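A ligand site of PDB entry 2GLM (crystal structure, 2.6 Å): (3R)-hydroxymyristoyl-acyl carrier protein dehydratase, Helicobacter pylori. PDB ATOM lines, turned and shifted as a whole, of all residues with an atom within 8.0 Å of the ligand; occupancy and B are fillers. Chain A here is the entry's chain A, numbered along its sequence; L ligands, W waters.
Water W1 bridges NE2 of Gln 52 and N1 of the ligand.
Residues that only touch the ligand: Val 137.
Of the 14 residues printed, 3 come within 4 Å of the ligand.
The nearest printed residue that does not touch the ligand is Leu 138 (4.2 Å).
O of Gln 52 lies close to N2 of the ligand (3.5 Å).
The side-chain amide nitrogen of Gln 52 sits close to a nitrogen (N2) of the ligand, at 2.7 Å.
OE2 of Glu 136 is in salt-bridge range of N1 of the ligand, 2.8 Å away.
The backbone carbonyl oxygen (O) of Gln 52 is in hydrogen-bond range of the backbone NH (N) of Val 137 (2.6 Å).
The backbone NH of Glu 136 is in hydrogen-bond range of the backbone carbonyl oxygen of Gly 148 (2.8 Å).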
ATOM      1  N   GLN A  49       4.163 -26.464  21.983  1.00  0.00           N
ATOM      2  CA  GLN A  49       3.205 -26.222  23.059  1.00  0.00           C
ATOM      3  C   GLN A  49       2.999 -24.722  23.214  1.00  0.00           C
ATOM      4  O   GLN A  49       3.884 -24.018  23.704  1.00  0.00           O
ATOM      5  CB  GLN A  49       3.716 -26.825  24.377  1.00  0.00           C
ATOM      6  CG  GLN A  49       3.002 -26.306  25.616  1.00  0.00           C
ATOM      7  CD  GLN A  49       1.484 -26.523  25.597  1.00  0.00           C
ATOM      8  OE1 GLN A  49       0.718 -25.630  25.982  1.00  0.00           O
ATOM      9  NE2 GLN A  49       1.040 -27.714  25.179  1.00  0.00           N
ATOM     10  N   ALA A  50       1.843 -24.236  22.781  1.00  0.00           N
ATOM     11  CA  ALA A  50       1.504 -22.815  22.845  1.00  0.00           C
ATOM     12  C   ALA A  50       1.941 -22.089  24.109  1.00  0.00           C
ATOM     13  O   ALA A  50       1.760 -22.579  25.231  1.00  0.00           O
ATOM     14  CB  ALA A  50       0.000 -22.631  22.643  1.00  0.00           C
ATOM     15  N   ASN A  51       2.510 -20.915  23.917  1.00  0.00           N
ATOM     16  CA  ASN A  51       2.954 -20.073  25.019  1.00  0.00           C
ATOM     17  C   ASN A  51       3.992 -20.715  25.924  1.00  0.00           C
ATOM     18  O   ASN A  51       4.382 -20.116  26.918  1.00  0.00           O
ATOM     19  CB  ASN A  51       1.754 -19.640  25.858  1.00  0.00           C
ATOM     20  CG  ASN A  51       0.682 -18.951  25.030  1.00  0.00           C
ATOM     21  OD1 ASN A  51      -0.393 -19.500  24.802  1.00  0.00           O
ATOM     22  ND2 ASN A  51       0.986 -17.746  24.574  1.00  0.00           N
ATOM     23  N   GLN A  52       4.441 -21.928  25.602  1.00  0.00           N
ATOM     24  CA  GLN A  52       5.419 -22.592  26.452  1.00  0.00           C
ATOM     25  C   GLN A  52       6.731 -22.931  25.777  1.00  0.00           C
ATOM     26  O   GLN A  52       7.791 -22.465  26.205  1.00  0.00           O
ATOM     27  CB  GLN A  52       4.838 -23.870  27.044  1.00  0.00           C
ATOM     28  CG  GLN A  52       3.681 -23.652  28.013  1.00  0.00           C
ATOM     29  CD  GLN A  52       3.585 -24.750  29.049  1.00  0.00           C
ATOM     30  OE1 GLN A  52       2.501 -25.119  29.475  1.00  0.00           O
ATOM     31  NE2 GLN A  52       4.737 -25.254  29.476  1.00  0.00           N
ATOM     32  N   LYS A  53       6.691 -23.740  24.737  1.00  0.00           N
ATOM     33  CA  LYS A  53       7.931 -24.123  24.083  1.00  0.00           C
ATOM     34  C   LYS A  53       7.763 -24.684  22.704  1.00  0.00           C
ATOM     35  O   LYS A  53       6.649 -24.942  22.237  1.00  0.00           O
ATOM     36  CB  LYS A  53       8.679 -25.172  24.898  1.00  0.00           C
ATOM     37  CG  LYS A  53       8.039 -26.539  24.839  1.00  0.00           C
ATOM     38  CD  LYS A  53       9.026 -27.599  25.270  1.00  0.00           C
ATOM     39  CE  LYS A  53       8.381 -28.970  25.327  1.00  0.00           C
ATOM     40  NZ  LYS A  53       9.333 -29.986  25.888  1.00  0.00           N
ATOM     41  N   ILE A  54       8.916 -24.890  22.069  1.00  0.00           N
ATOM     42  CA  ILE A  54       8.987 -25.473  20.743  1.00  0.00           C
ATOM     43  C   ILE A  54      10.349 -26.163  20.616  1.00  0.00           C
ATOM     44  O   ILE A  54      11.351 -25.680  21.139  1.00  0.00           O
ATOM     45  CB  ILE A  54       8.798 -24.378  19.633  1.00  0.00           C
ATOM     46  CG1 ILE A  54       8.777 -25.025  18.242  1.00  0.00           C
ATOM     47  CG2 ILE A  54       9.896 -23.338  19.723  1.00  0.00           C
ATOM     48  CD1 ILE A  54       8.526 -24.048  17.106  1.00  0.00           C
ATOM     49  N   LEU A 135      13.518 -24.068  22.361  1.00  0.00           N
ATOM     50  CA  LEU A 135      13.170 -22.745  22.869  1.00  0.00           C
ATOM     51  C   LEU A 135      11.985 -22.797  23.827  1.00  0.00           C
ATOM     52  O   LEU A 135      10.953 -23.397  23.524  1.00  0.00           O
ATOM     53  CB  LEU A 135      12.827 -21.795  21.720  1.00  0.00           C
ATOM     54  CG  LEU A 135      13.963 -21.269  20.835  1.00  0.00           C
ATOM     55  CD1 LEU A 135      15.001 -20.571  21.701  1.00  0.00           C
ATOM     56  CD2 LEU A 135      14.590 -22.415  20.035  1.00  0.00           C
ATOM     57  N   GLU A 136      12.126 -22.161  24.992  1.00  0.00           N
ATOM     58  CA  GLU A 136      11.047 -22.103  25.966  1.00  0.00           C
ATOM     59  C   GLU A 136      10.641 -20.634  26.064  1.00  0.00           C
ATOM     60  O   GLU A 136      11.449 -19.744  25.839  1.00  0.00           O
ATOM     61  CB  GLU A 136      11.516 -22.589  27.354  1.00  0.00           C
ATOM     62  CG  GLU A 136      12.323 -23.911  27.398  1.00  0.00           C
ATOM     63  CD  GLU A 136      11.495 -25.175  27.664  1.00  0.00           C
ATOM     64  OE1 GLU A 136      12.081 -26.170  28.166  1.00  0.00           O
ATOM     65  OE2 GLU A 136      10.273 -25.207  27.383  1.00  0.00           O
ATOM     66  N   VAL A 137       9.369 -20.374  26.388  1.00  0.00           N
ATOM     67  CA  VAL A 137       8.889 -19.000  26.538  1.00  0.00           C
ATOM     68  C   VAL A 137       9.181 -18.468  27.947  1.00  0.00           C
ATOM     69  O   VAL A 137       8.593 -18.914  28.938  1.00  0.00           O
ATOM     70  CB  VAL A 137       7.386 -18.927  26.276  1.00  0.00           C
ATOM     71  CG1 VAL A 137       6.881 -17.520  26.544  1.00  0.00           C
ATOM     72  CG2 VAL A 137       7.090 -19.338  24.864  1.00  0.00           C
ATOM     73  N   LEU A 138      10.092 -17.511  28.036  1.00  0.00           N
ATOM     74  CA  LEU A 138      10.457 -16.935  29.317  1.00  0.00           C
ATOM     75  C   LEU A 138       9.470 -15.855  29.759  1.00  0.00           C
ATOM     76  O   LEU A 138       9.279 -15.644  30.956  1.00  0.00           O
ATOM     77  CB  LEU A 138      11.859 -16.343  29.234  1.00  0.00           C
ATOM     78  CG  LEU A 138      12.957 -17.363  28.958  1.00  0.00           C
ATOM     79  CD1 LEU A 138      14.212 -16.624  28.525  1.00  0.00           C
ATOM     80  CD2 LEU A 138      13.198 -18.200  30.201  1.00  0.00           C
ATOM     81  N   LYS A 139       8.848 -15.189  28.799  1.00  0.00           N
ATOM     82  CA  LYS A 139       7.908 -14.112  29.115  1.00  0.00           C
ATOM     83  C   LYS A 139       7.227 -13.611  27.840  1.00  0.00           C
ATOM     84  O   LYS A 139       7.875 -13.440  26.819  1.00  0.00           O
ATOM     85  CB  LYS A 139       8.680 -12.981  29.807  1.00  0.00           C
ATOM     86  CG  LYS A 139       7.881 -11.743  30.151  1.00  0.00           C
ATOM     87  CD  LYS A 139       8.722 -10.791  31.012  1.00  0.00           C
ATOM     88  CE  LYS A 139       8.115  -9.388  31.099  1.00  0.00           C
ATOM     89  NZ  LYS A 139       8.139  -8.678  29.783  1.00  0.00           N
ATOM     90  N   GLN A 146       9.856 -13.008  24.850  1.00  0.00           N
ATOM     91  CA  GLN A 146      11.189 -13.291  25.353  1.00  0.00           C
ATOM     92  C   GLN A 146      11.326 -14.798  25.509  1.00  0.00           C
ATOM     93  O   GLN A 146      10.590 -15.418  26.284  1.00  0.00           O
ATOM     94  CB  GLN A 146      11.399 -12.588  26.695  1.00  0.00           C
ATOM     95  CG  GLN A 146      11.386 -11.076  26.567  1.00  0.00           C
ATOM     96  CD  GLN A 146      11.198 -10.357  27.892  1.00  0.00           C
ATOM     97  OE1 GLN A 146      12.027 -10.465  28.805  1.00  0.00           O
ATOM     98  NE2 GLN A 146      10.091  -9.608  28.012  1.00  0.00           N
ATOM     99  N   VAL A 147      12.255 -15.379  24.768  1.00  0.00           N
ATOM    100  CA  VAL A 147      12.476 -16.821  24.825  1.00  0.00           C
ATOM    101  C   VAL A 147      13.943 -17.149  25.035  1.00  0.00           C
ATOM    102  O   VAL A 147      14.822 -16.291  24.886  1.00  0.00           O
ATOM    103  CB  VAL A 147      12.024 -17.520  23.521  1.00  0.00           C
ATOM    104  CG1 VAL A 147      10.578 -17.163  23.207  1.00  0.00           C
ATOM    105  CG2 VAL A 147      12.937 -17.135  22.374  1.00  0.00           C
ATOM    106  N   GLY A 148      14.217 -18.395  25.381  1.00  0.00           N
ATOM    107  CA  GLY A 148      15.568 -18.816  25.598  1.00  0.00           C
ATOM    108  C   GLY A 148      15.661 -20.306  25.434  1.00  0.00           C
ATOM    109  O   GLY A 148      14.647 -21.007  25.497  1.00  0.00           O
HETATM  110  C1  LIG L   1       9.349 -23.511  30.216  1.00  0.00           C
HETATM  111  C2  LIG L   1      10.616 -24.060  30.590  1.00  0.00           C
HETATM  112  C3  LIG L   1      11.611 -23.220  31.114  1.00  0.00           C
HETATM  113  C4  LIG L   1      11.365 -21.843  31.280  1.00  0.00           C
HETATM  114  C5  LIG L   1      10.128 -21.295  30.915  1.00  0.00           C
HETATM  115  C6  LIG L   1       9.117 -22.126  30.377  1.00  0.00           C
HETATM  116  C7  LIG L   1       8.270 -24.405  29.654  1.00  0.00           C
HETATM  117  N1  LIG L   1       8.483 -25.678  29.494  1.00  0.00           N
HETATM  118  N2  LIG L   1       7.047 -23.874  29.299  1.00  0.00           N
HETATM  119  O   HOH W   1       5.966 -27.193  28.000  1.00  0.00           O
HETATM  120  O   HOH W   2      12.957 -20.957  34.017  1.00  0.00           O
